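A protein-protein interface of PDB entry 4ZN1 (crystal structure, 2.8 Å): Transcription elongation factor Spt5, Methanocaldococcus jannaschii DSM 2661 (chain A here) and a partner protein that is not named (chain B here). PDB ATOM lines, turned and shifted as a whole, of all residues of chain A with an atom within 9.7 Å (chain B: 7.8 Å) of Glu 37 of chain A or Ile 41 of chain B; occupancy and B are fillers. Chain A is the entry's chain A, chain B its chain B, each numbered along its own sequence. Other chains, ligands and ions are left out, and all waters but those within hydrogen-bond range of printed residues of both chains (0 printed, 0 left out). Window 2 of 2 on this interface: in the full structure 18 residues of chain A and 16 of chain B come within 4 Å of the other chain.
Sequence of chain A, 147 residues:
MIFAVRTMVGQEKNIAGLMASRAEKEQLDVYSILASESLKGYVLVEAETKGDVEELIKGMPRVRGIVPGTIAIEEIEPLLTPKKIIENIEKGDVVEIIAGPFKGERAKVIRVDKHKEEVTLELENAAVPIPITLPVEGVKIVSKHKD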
ATOM      1  N   VAL A   9       7.261   4.022 -24.289  1.00  0.00           N
ATOM      2  CA  VAL A   9       5.868   4.231 -23.893  1.00  0.00           C
ATOM      3  C   VAL A   9       4.999   3.667 -24.995  1.00  0.00           C
ATOM      4  O   VAL A   9       5.322   3.792 -26.172  1.00  0.00           O
ATOM      5  CB  VAL A   9       5.535   5.722 -23.647  1.00  0.00           C
ATOM      6  CG1 VAL A   9       4.053   5.914 -23.329  1.00  0.00           C
ATOM      7  CG2 VAL A   9       6.388   6.275 -22.509  1.00  0.00           C
ATOM      8  N   GLY A  10       3.907   3.032 -24.598  1.00  0.00           N
ATOM      9  CA  GLY A  10       3.021   2.364 -25.535  1.00  0.00           C
ATOM     10  C   GLY A  10       3.490   1.024 -26.088  1.00  0.00           C
ATOM     11  O   GLY A  10       2.812   0.463 -26.949  1.00  0.00           O
ATOM     12  N   GLU A  12       4.537  -1.499 -23.767  1.00  0.00           N
ATOM     13  CA  GLU A  12       4.690  -2.204 -22.506  1.00  0.00           C
ATOM     14  C   GLU A  12       4.112  -3.597 -22.677  1.00  0.00           C
ATOM     15  O   GLU A  12       4.790  -4.580 -22.406  1.00  0.00           O
ATOM     16  CB  GLU A  12       3.981  -1.452 -21.364  1.00  0.00           C
ATOM     17  CG  GLU A  12       4.464  -0.009 -21.158  1.00  0.00           C
ATOM     18  CD  GLU A  12       3.706   1.023 -21.990  1.00  0.00           C
ATOM     19  OE1 GLU A  12       2.822   0.645 -22.787  1.00  0.00           O
ATOM     20  OE2 GLU A  12       4.000   2.230 -21.872  1.00  0.00           O
ATOM     21  N   LYS A  13       2.873  -3.667 -23.160  1.00  0.00           N
ATOM     22  CA  LYS A  13       2.203  -4.952 -23.478  1.00  0.00           C
ATOM     23  C   LYS A  13       2.925  -5.815 -24.512  1.00  0.00           C
ATOM     24  O   LYS A  13       2.961  -7.041 -24.381  1.00  0.00           O
ATOM     25  CB  LYS A  13       0.754  -4.719 -23.954  1.00  0.00           C
ATOM     26  CG  LYS A  13      -0.277  -4.822 -22.834  1.00  0.00           C
ATOM     27  CD  LYS A  13      -1.509  -3.943 -23.037  1.00  0.00           C
ATOM     28  CE  LYS A  13      -2.117  -3.505 -21.702  1.00  0.00           C
ATOM     29  NZ  LYS A  13      -1.291  -2.490 -20.973  1.00  0.00           N
ATOM     30  N   LEU A  34       3.592  -7.685 -15.205  1.00  0.00           N
ATOM     31  CA  LEU A  34       2.458  -6.785 -15.071  1.00  0.00           C
ATOM     32  C   LEU A  34       2.629  -5.503 -15.901  1.00  0.00           C
ATOM     33  O   LEU A  34       3.638  -4.809 -15.788  1.00  0.00           O
ATOM     34  CB  LEU A  34       2.266  -6.441 -13.603  1.00  0.00           C
ATOM     35  CG  LEU A  34       1.062  -5.575 -13.248  1.00  0.00           C
ATOM     36  CD1 LEU A  34      -0.247  -6.196 -13.695  1.00  0.00           C
ATOM     37  CD2 LEU A  34       1.038  -5.372 -11.749  1.00  0.00           C
ATOM     38  N   ALA A  35       1.628  -5.211 -16.734  1.00  0.00           N
ATOM     39  CA  ALA A  35       1.588  -4.008 -17.548  1.00  0.00           C
ATOM     40  C   ALA A  35       0.245  -3.349 -17.304  1.00  0.00           C
ATOM     41  O   ALA A  35      -0.788  -3.880 -17.714  1.00  0.00           O
ATOM     42  CB  ALA A  35       1.754  -4.359 -19.014  1.00  0.00           C
ATOM     43  N   SER A  36       0.263  -2.218 -16.600  1.00  0.00           N
ATOM     44  CA  SER A  36      -0.948  -1.431 -16.339  1.00  0.00           C
ATOM     45  C   SER A  36      -0.992  -0.208 -17.241  1.00  0.00           C
ATOM     46  O   SER A  36       0.043   0.413 -17.499  1.00  0.00           O
ATOM     47  CB  SER A  36      -1.008  -0.980 -14.880  1.00  0.00           C
ATOM     48  OG  SER A  36      -2.287  -0.442 -14.579  1.00  0.00           O
ATOM     49  N   GLU A  37      -2.195   0.130 -17.709  1.00  0.00           N
ATOM     50  CA  GLU A  37      -2.419   1.325 -18.534  1.00  0.00           C
ATOM     51  C   GLU A  37      -1.960   2.603 -17.802  1.00  0.00           C
ATOM     52  O   GLU A  37      -1.368   3.501 -18.416  1.00  0.00           O
ATOM     53  CB  GLU A  37      -3.899   1.422 -18.932  1.00  0.00           C
ATOM     54  N   SER A  38      -2.195   2.632 -16.483  1.00  0.00           N
ATOM     55  CA  SER A  38      -1.791   3.737 -15.586  1.00  0.00           C
ATOM     56  C   SER A  38      -0.280   3.927 -15.411  1.00  0.00           C
ATOM     57  O   SER A  38       0.163   4.989 -14.978  1.00  0.00           O
ATOM     58  CB  SER A  38      -2.409   3.531 -14.194  1.00  0.00           C
ATOM     59  N   LEU A  39       0.499   2.900 -15.749  1.00  0.00           N
ATOM     60  CA  LEU A  39       1.928   2.816 -15.471  1.00  0.00           C
ATOM     61  C   LEU A  39       2.660   2.773 -16.812  1.00  0.00           C
ATOM     62  O   LEU A  39       3.325   1.795 -17.143  1.00  0.00           O
ATOM     63  CB  LEU A  39       2.154   1.528 -14.652  1.00  0.00           C
ATOM     64  CG  LEU A  39       3.116   1.422 -13.467  1.00  0.00           C
ATOM     65  CD1 LEU A  39       3.026   2.627 -12.548  1.00  0.00           C
ATOM     66  CD2 LEU A  39       2.800   0.147 -12.689  1.00  0.00           C
ATOM     67  N   LYS A  40       2.514   3.838 -17.594  1.00  0.00           N
ATOM     68  CA  LYS A  40       3.052   3.888 -18.959  1.00  0.00           C
ATOM     69  C   LYS A  40       4.555   4.112 -18.914  1.00  0.00           C
ATOM     70  O   LYS A  40       5.026   4.933 -18.126  1.00  0.00           O
ATOM     71  CB  LYS A  40       2.382   5.006 -19.764  1.00  0.00           C
ATOM     72  N   GLY A  41       5.290   3.380 -19.758  1.00  0.00           N
ATOM     73  CA  GLY A  41       6.764   3.365 -19.767  1.00  0.00           C
ATOM     74  C   GLY A  41       7.416   2.260 -18.942  1.00  0.00           C
ATOM     75  O   GLY A  41       8.617   2.023 -19.068  1.00  0.00           O
ATOM     76  N   TYR A  42       6.621   1.591 -18.102  1.00  0.00           N
ATOM     77  CA  TYR A  42       7.095   0.603 -17.141  1.00  0.00           C
ATOM     78  C   TYR A  42       6.345  -0.693 -17.355  1.00  0.00           C
ATOM     79  O   TYR A  42       5.112  -0.700 -17.532  1.00  0.00           O
ATOM     80  CB  TYR A  42       6.854   1.068 -15.692  1.00  0.00           C
ATOM     81  CG  TYR A  42       7.631   2.298 -15.336  1.00  0.00           C
ATOM     82  CD1 TYR A  42       8.934   2.209 -14.865  1.00  0.00           C
ATOM     83  CD2 TYR A  42       7.078   3.563 -15.508  1.00  0.00           C
ATOM     84  CE1 TYR A  42       9.661   3.353 -14.568  1.00  0.00           C
ATOM     85  CE2 TYR A  42       7.798   4.708 -15.220  1.00  0.00           C
ATOM     86  CZ  TYR A  42       9.086   4.600 -14.753  1.00  0.00           C
ATOM     87  OH  TYR A  42       9.780   5.748 -14.466  1.00  0.00           O
ATOM     88  N   VAL A  43       7.103  -1.783 -17.327  1.00  0.00           N
ATOM     89  CA  VAL A  43       6.549  -3.116 -17.227  1.00  0.00           C
ATOM     90  C   VAL A  43       7.119  -3.684 -15.947  1.00  0.00           C
ATOM     91  O   VAL A  43       8.322  -3.772 -15.802  1.00  0.00           O
ATOM     92  CB  VAL A  43       6.966  -3.977 -18.419  1.00  0.00           C
ATOM     93  CG1 VAL A  43       6.383  -5.370 -18.284  1.00  0.00           C
ATOM     94  CG2 VAL A  43       6.483  -3.358 -19.722  1.00  0.00           C
ATOM     95  N   LEU A  79      -3.267  -1.594  -8.303  1.00  0.00           N
ATOM     96  CA  LEU A  79      -3.349  -2.036  -9.688  1.00  0.00           C
ATOM     97  C   LEU A  79      -3.884  -3.473  -9.865  1.00  0.00           C
ATOM     98  O   LEU A  79      -4.433  -3.791 -10.918  1.00  0.00           O
ATOM     99  CB  LEU A  79      -1.967  -1.907 -10.350  1.00  0.00           C
ATOM    100  N   PRO A  82      -8.842  -3.846  -8.852  1.00  0.00           N
ATOM    101  CA  PRO A  82      -9.945  -2.900  -9.139  1.00  0.00           C
ATOM    102  C   PRO A  82     -11.357  -3.482  -8.912  1.00  0.00           C
ATOM    103  O   PRO A  82     -12.020  -3.156  -7.920  1.00  0.00           O
ATOM    104  CB  PRO A  82      -9.741  -2.556 -10.629  1.00  0.00           C
ATOM    105  CG  PRO A  82      -8.320  -2.900 -10.922  1.00  0.00           C
ATOM    106  CD  PRO A  82      -8.030  -4.097 -10.064  1.00  0.00           C
ATOM    107  N   GLU A 117     -21.845   0.203 -18.072  1.00  0.00           N
ATOM    108  CA  GLU A 117     -21.118   0.651 -16.884  1.00  0.00           C
ATOM    109  C   GLU A 117     -21.312   2.152 -16.729  1.00  0.00           C
ATOM    110  O   GLU A 117     -20.377   2.898 -16.420  1.00  0.00           O
ATOM    111  CB  GLU A 117     -19.641   0.219 -16.943  1.00  0.00           C
ATOM    112  CG  GLU A 117     -19.177  -0.522 -15.693  1.00  0.00           C
ATOM    113  CD  GLU A 117     -18.075  -1.524 -15.977  1.00  0.00           C
ATOM    114  OE1 GLU A 117     -18.377  -2.738 -16.074  1.00  0.00           O
ATOM    115  OE2 GLU A 117     -16.914  -1.086 -16.118  1.00  0.00           O
ATOM    116  N   GLU A 137     -17.284   5.466 -12.991  1.00  0.00           N
ATOM    117  CA  GLU A 137     -15.985   6.154 -12.807  1.00  0.00           C
ATOM    118  C   GLU A 137     -16.077   7.619 -12.418  1.00  0.00           C
ATOM    119  O   GLU A 137     -15.308   8.084 -11.584  1.00  0.00           O
ATOM    120  CB  GLU A 137     -15.180   6.116 -14.113  1.00  0.00           C
ATOM    121  CG  GLU A 137     -14.006   5.158 -14.153  1.00  0.00           C
ATOM    122  CD  GLU A 137     -13.182   5.365 -15.416  1.00  0.00           C
ATOM    123  OE1 GLU A 137     -13.715   5.086 -16.517  1.00  0.00           O
ATOM    124  OE2 GLU A 137     -12.019   5.828 -15.312  1.00  0.00           O
ATOM    125  N   ALA B  16     -11.137 -10.768 -23.582  1.00  0.00           N
ATOM    126  CA  ALA B  16     -10.969 -11.058 -22.169  1.00  0.00           C
ATOM    127  C   ALA B  16     -12.298 -11.498 -21.557  1.00  0.00           C
ATOM    128  O   ALA B  16     -13.305 -10.796 -21.716  1.00  0.00           O
ATOM    129  CB  ALA B  16     -10.441  -9.828 -21.458  1.00  0.00           C
ATOM    130  N   LYS B  21     -11.285 -12.756 -16.364  1.00  0.00           N
ATOM    131  CA  LYS B  21     -10.299 -11.873 -17.039  1.00  0.00           C
ATOM    132  C   LYS B  21      -9.264 -12.588 -17.930  1.00  0.00           C
ATOM    133  O   LYS B  21      -8.364 -11.936 -18.467  1.00  0.00           O
ATOM    134  CB  LYS B  21      -9.595 -10.906 -16.041  1.00  0.00           C
ATOM    135  CG  LYS B  21     -10.345  -9.601 -15.795  1.00  0.00           C
ATOM    136  CD  LYS B  21      -9.778  -8.757 -14.656  1.00  0.00           C
ATOM    137  CE  LYS B  21     -10.080  -9.313 -13.267  1.00  0.00           C
ATOM    138  NZ  LYS B  21     -11.489  -9.758 -13.059  1.00  0.00           N
ATOM    139  N   LEU B  23      -7.368 -14.164 -20.970  1.00  0.00           N
ATOM    140  CA  LEU B  23      -7.287 -13.711 -22.347  1.00  0.00           C
ATOM    141  C   LEU B  23      -7.323 -14.867 -23.336  1.00  0.00           C
ATOM    142  O   LEU B  23      -6.501 -15.794 -23.273  1.00  0.00           O
ATOM    143  CB  LEU B  23      -6.019 -12.901 -22.591  1.00  0.00           C
ATOM    144  CG  LEU B  23      -5.865 -11.551 -21.908  1.00  0.00           C
ATOM    145  CD1 LEU B  23      -4.641 -10.843 -22.476  1.00  0.00           C
ATOM    146  CD2 LEU B  23      -7.093 -10.684 -22.104  1.00  0.00           C
ATOM    147  N   GLU B  38     -14.122  -7.657 -25.989  1.00  0.00           N
ATOM    148  CA  GLU B  38     -12.946  -6.998 -26.533  1.00  0.00           C
ATOM    149  C   GLU B  38     -12.531  -5.774 -25.706  1.00  0.00           C
ATOM    150  O   GLU B  38     -11.382  -5.341 -25.808  1.00  0.00           O
ATOM    151  CB  GLU B  38     -13.179  -6.579 -27.995  1.00  0.00           C
ATOM    152  CG  GLU B  38     -13.138  -7.720 -29.007  1.00  0.00           C
ATOM    153  CD  GLU B  38     -12.798  -7.236 -30.410  1.00  0.00           C
ATOM    154  OE1 GLU B  38     -13.299  -6.156 -30.814  1.00  0.00           O
ATOM    155  OE2 GLU B  38     -12.021  -7.934 -31.101  1.00  0.00           O
ATOM    156  N   ASN B  39     -13.442  -5.218 -24.901  1.00  0.00           N
ATOM    157  CA  ASN B  39     -13.183  -3.952 -24.204  1.00  0.00           C
ATOM    158  C   ASN B  39     -12.487  -4.195 -22.862  1.00  0.00           C
ATOM    159  O   ASN B  39     -13.062  -3.971 -21.784  1.00  0.00           O
ATOM    160  CB  ASN B  39     -14.482  -3.136 -24.045  1.00  0.00           C
ATOM    161  CG  ASN B  39     -14.232  -1.678 -23.663  1.00  0.00           C
ATOM    162  OD1 ASN B  39     -13.090  -1.220 -23.542  1.00  0.00           O
ATOM    163  ND2 ASN B  39     -15.315  -0.940 -23.472  1.00  0.00           N
ATOM    164  N   TRP B  40     -11.229  -4.629 -22.955  1.00  0.00           N
ATOM    165  CA  TRP B  40     -10.419  -4.977 -21.790  1.00  0.00           C
ATOM    166  C   TRP B  40      -9.147  -4.149 -21.774  1.00  0.00           C
ATOM    167  O   TRP B  40      -8.647  -3.742 -22.813  1.00  0.00           O
ATOM    168  CB  TRP B  40     -10.118  -6.481 -21.758  1.00  0.00           C
ATOM    169  CG  TRP B  40      -9.307  -6.961 -22.899  1.00  0.00           C
ATOM    170  CD1 TRP B  40      -9.764  -7.493 -24.065  1.00  0.00           C
ATOM    171  CD2 TRP B  40      -7.880  -6.951 -22.991  1.00  0.00           C
ATOM    172  NE1 TRP B  40      -8.710  -7.806 -24.887  1.00  0.00           N
ATOM    173  CE2 TRP B  40      -7.541  -7.487 -24.251  1.00  0.00           C
ATOM    174  CE3 TRP B  40      -6.851  -6.534 -22.128  1.00  0.00           C
ATOM    175  CZ2 TRP B  40      -6.216  -7.627 -24.670  1.00  0.00           C
ATOM    176  CZ3 TRP B  40      -5.534  -6.666 -22.549  1.00  0.00           C
ATOM    177  CH2 TRP B  40      -5.228  -7.210 -23.805  1.00  0.00           C
ATOM    178  N   ILE B  41      -8.632  -3.910 -20.575  1.00  0.00           N
ATOM    179  CA  ILE B  41      -7.572  -2.944 -20.348  1.00  0.00           C
ATOM    180  C   ILE B  41      -6.554  -3.546 -19.379  1.00  0.00           C
ATOM    181  O   ILE B  41      -6.929  -4.263 -18.449  1.00  0.00           O
ATOM    182  CB  ILE B  41      -8.176  -1.634 -19.784  1.00  0.00           C
ATOM    183  CG1 ILE B  41      -9.083  -0.963 -20.830  1.00  0.00           C
ATOM    184  CG2 ILE B  41      -7.099  -0.633 -19.390  1.00  0.00           C
ATOM    185  CD1 ILE B  41     -10.195  -0.117 -20.241  1.00  0.00           C
ATOM    186  N   GLY B  42      -5.269  -3.262 -19.611  1.00  0.00           N
ATOM    187  CA  GLY B  42      -4.185  -3.712 -18.730  1.00  0.00           C
ATOM    188  C   GLY B  42      -3.875  -5.184 -18.906  1.00  0.00           C
ATOM    189  O   GLY B  42      -4.682  -5.913 -19.477  1.00  0.00           O
ATOM    190  N   LEU B  43      -2.722  -5.634 -18.410  1.00  0.00           N
ATOM    191  CA  LEU B  43      -2.278  -7.022 -18.653  1.00  0.00           C
ATOM    192  C   LEU B  43      -1.403  -7.606 -17.559  1.00  0.00           C
ATOM    193  O   LEU B  43      -0.389  -7.023 -17.218  1.00  0.00           O
ATOM    194  CB  LEU B  43      -1.522  -7.094 -19.981  1.00  0.00           C
ATOM    195  CG  LEU B  43      -0.594  -8.285 -20.268  1.00  0.00           C
ATOM    196  CD1 LEU B  43      -1.309  -9.376 -21.043  1.00  0.00           C
ATOM    197  CD2 LEU B  43       0.621  -7.814 -21.040  1.00  0.00           C
ATOM    198  N   LEU B  44      -1.796  -8.780 -17.065  1.00  0.00           N
ATOM    199  CA  LEU B  44      -1.039  -9.550 -16.085  1.00  0.00           C
ATOM    200  C   LEU B  44      -0.761 -10.907 -16.679  1.00  0.00           C
ATOM    201  O   LEU B  44      -1.681 -11.664 -16.971  1.00  0.00           O
ATOM    202  CB  LEU B  44      -1.844  -9.746 -14.798  1.00  0.00           C
ATOM    203  CG  LEU B  44      -1.121 -10.009 -13.462  1.00  0.00           C
ATOM    204  CD1 LEU B  44      -1.964 -10.939 -12.611  1.00  0.00           C
ATOM    205  CD2 LEU B  44       0.286 -10.564 -13.571  1.00  0.00           C
ATOM    206  N   TYR B  66      -3.848 -12.398 -18.551  1.00  0.00           N
ATOM    207  CA  TYR B  66      -5.081 -11.895 -17.942  1.00  0.00           C
ATOM    208  C   TYR B  66      -5.192 -10.401 -18.155  1.00  0.00           C
ATOM    209  O   TYR B  66      -4.204  -9.697 -18.029  1.00  0.00           O
ATOM    210  CB  TYR B  66      -5.076 -12.156 -16.437  1.00  0.00           C
ATOM    211  CG  TYR B  66      -5.267 -13.598 -16.041  1.00  0.00           C
ATOM    212  CD1 TYR B  66      -6.540 -14.152 -15.957  1.00  0.00           C
ATOM    213  CD2 TYR B  66      -4.176 -14.405 -15.734  1.00  0.00           C
ATOM    214  CE1 TYR B  66      -6.722 -15.476 -15.591  1.00  0.00           C
ATOM    215  CE2 TYR B  66      -4.346 -15.728 -15.362  1.00  0.00           C
ATOM    216  CZ  TYR B  66      -5.617 -16.260 -15.294  1.00  0.00           C
ATOM    217  OH  TYR B  66      -5.762 -17.570 -14.925  1.00  0.00           O
ATOM    218  N   ALA B  67      -6.392  -9.914 -18.448  1.00  0.00           N
ATOM    219  CA  ALA B  67      -6.644  -8.471 -18.439  1.00  0.00           C
ATOM    220  C   ALA B  67      -6.694  -7.956 -16.996  1.00  0.00           C
ATOM    221  O   ALA B  67      -6.846  -8.732 -16.057  1.00  0.00           O
ATOM    222  CB  ALA B  67      -7.942  -8.153 -19.160  1.00  0.00           C
ATOM    223  N   LEU B  68      -6.550  -6.651 -16.817  1.00  0.00           N
ATOM    224  CA  LEU B  68      -6.675  -6.044 -15.487  1.00  0.00           C
ATOM    225  C   LEU B  68      -8.069  -5.444 -15.244  1.00  0.00           C
ATOM    226  O   LEU B  68      -8.553  -5.436 -14.105  1.00  0.00           O
ATOM    227  CB  LEU B  68      -5.576  -4.998 -15.276  1.00  0.00           C
ATOM    228  CG  LEU B  68      -4.156  -5.548 -15.179  1.00  0.00           C
ATOM    229  CD1 LEU B  68      -3.135  -4.428 -15.157  1.00  0.00           C
ATOM    230  CD2 LEU B  68      -3.987  -6.404 -13.941  1.00  0.00           C
ATOM    231  N   SER B  69      -8.692  -4.933 -16.308  1.00  0.00           N
ATOM    232  CA  SER B  69     -10.083  -4.485 -16.279  1.00  0.00           C
ATOM    233  C   SER B  69     -10.789  -4.967 -17.527  1.00  0.00           C
ATOM    234  O   SER B  69     -10.150  -5.126 -18.563  1.00  0.00           O
ATOM    235  CB  SER B  69     -10.144  -2.964 -16.218  1.00  0.00           C
ATOM    236  OG  SER B  69      -9.943  -2.510 -14.895  1.00  0.00           O
ATOM    237  N   VAL B  70     -12.096  -5.221 -17.418  1.00  0.00           N
ATOM    238  CA  VAL B  70     -12.923  -5.658 -18.564  1.00  0.00           C
ATOM    239  C   VAL B  70     -14.346  -5.120 -18.469  1.00  0.00           C
ATOM    240  O   VAL B  70     -14.936  -5.055 -17.386  1.00  0.00           O
ATOM    241  CB  VAL B  70     -13.034  -7.202 -18.707  1.00  0.00           C
ATOM    242  CG1 VAL B  70     -13.610  -7.603 -20.068  1.00  0.00           C
ATOM    243  CG2 VAL B  70     -11.684  -7.865 -18.533  1.00  0.00           C
ATOM    244  N   LYS B  71     -14.884  -4.794 -19.640  1.00  0.00           N
ATOM    245  CA  LYS B  71     -16.203  -4.227 -19.808  1.00  0.00           C
ATOM    246  C   LYS B  71     -16.775  -4.773 -21.131  1.00  0.00           C
ATOM    247  O   LYS B  71     -16.037  -5.349 -21.932  1.00  0.00           O
ATOM    248  CB  LYS B  71     -16.049  -2.709 -19.886  1.00  0.00           C
ATOM    249  CG  LYS B  71     -17.175  -1.907 -19.263  1.00  0.00           C
ATOM    250  CD  LYS B  71     -17.572  -0.727 -20.143  1.00  0.00           C
ATOM    251  CE  LYS B  71     -16.447   0.294 -20.296  1.00  0.00           C
ATOM    252  NZ  LYS B  71     -16.293   1.138 -19.071  1.00  0.00           N
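N of Leu 43 of chain B lies within hydrogen-bond range of O of Ala 35 of chain A, 2.7 Å away. The side-chain amino group of Lys 71 of chain B is in salt-bridge range of the side-chain carboxylate of Glu 117 of chain A (3.7 Å).
O of Asn 39 of chain B is in hydrogen-bond range of N of Lys 71 of chain B (2.9 Å). O of Ile 41 of chain B lies within hydrogen-bond range of N of Leu 68 of chain B, 2.9 Å away. N of Ile 41 of chain B sits at hydrogen-bond distance from O of Ser 69 of chain B, at 2.8 Å. The backbone NH (N) of Leu 68 of chain B sits at hydrogen-bond distance from the backbone carbonyl oxygen (O) of Gly 42 of chain B (3.3 Å). The backbone NH (N) of Leu 44 of chain B lies within hydrogen-bond range of the backbone carbonyl oxygen (O) of Tyr 66 of chain B (2.8 Å).
CA of Gly 42 of chain B touches CE of Lys 13 of chain A, 3.6 Å away. CG of Lys 13 of chain A touches CD2 of Leu 43 of chain B (3.6 Å). Leu 34 of chain A touches Leu 43 of chain B. CD1 of Leu 34 of chain A touches CG of Leu 44 of chain B (3.9 Å). CD1 of Leu 34 of chain A touches CD1 of Leu 68 of chain B, at 3.7 Å. O of Ala 35 of chain A touches CA of Gly 42 of chain B, 3.5 Å away. O of Ala 35 of chain A touches CD1 of Leu 68 of chain B (3.5 Å). Ser 36 of chain A touches Leu 68 of chain B (CA to CD1, 3.9 Å). Glu 37 of chain A touches Ile 41 of chain B (CB to CG2, 3.8 Å).
Of the printed residues of chain B, Lys 13 of chain A touches Gly 42 and Leu 43. Printed residues of chain B within 4 Å of Leu 34 of chain A: Leu 43, Leu 44 and Leu 68. Of the printed residues of chain B, Ser 36 of chain A touches Leu 68. Of chain B, only Ile 41 comes within 4 Å of Glu 37 of chain A. Ile 41 of chain B touches one residue of chain A. No residue of chain A comes within 4 Å of Ser 69 of chain B. The nearest residue of chain B that does not touch Glu 37 of chain A is Gly 42 of chain B (4.4 Å). The nearest residue of chain A that does not touch Ile 41 of chain B is Lys 13 of chain A (5.0 Å).
Of the 16 printed residues of chain B, 6 touch a printed residue of chain A. Hydrophobic or aromatic side chains of chain B that line the printed part of chain A: Ile 41, Leu 43, Leu 44 and Leu 68. Printed residues of chain A that touch a printed residue of chain B: Lys 13, Leu 34, Ala 35, Ser 36, Glu 37 and Glu 117. Hydrophobic or aromatic side chains of chain A within 4 Å of the printed part of chain B: Leu 34 and Ala 35. Among the printed residues, Asp or Glu carboxylates within 4 Å of a Lys or Arg side-chain nitrogen of the other chain: Glu 117 of chain A with Lys 71 of chain B (3.7 Å).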
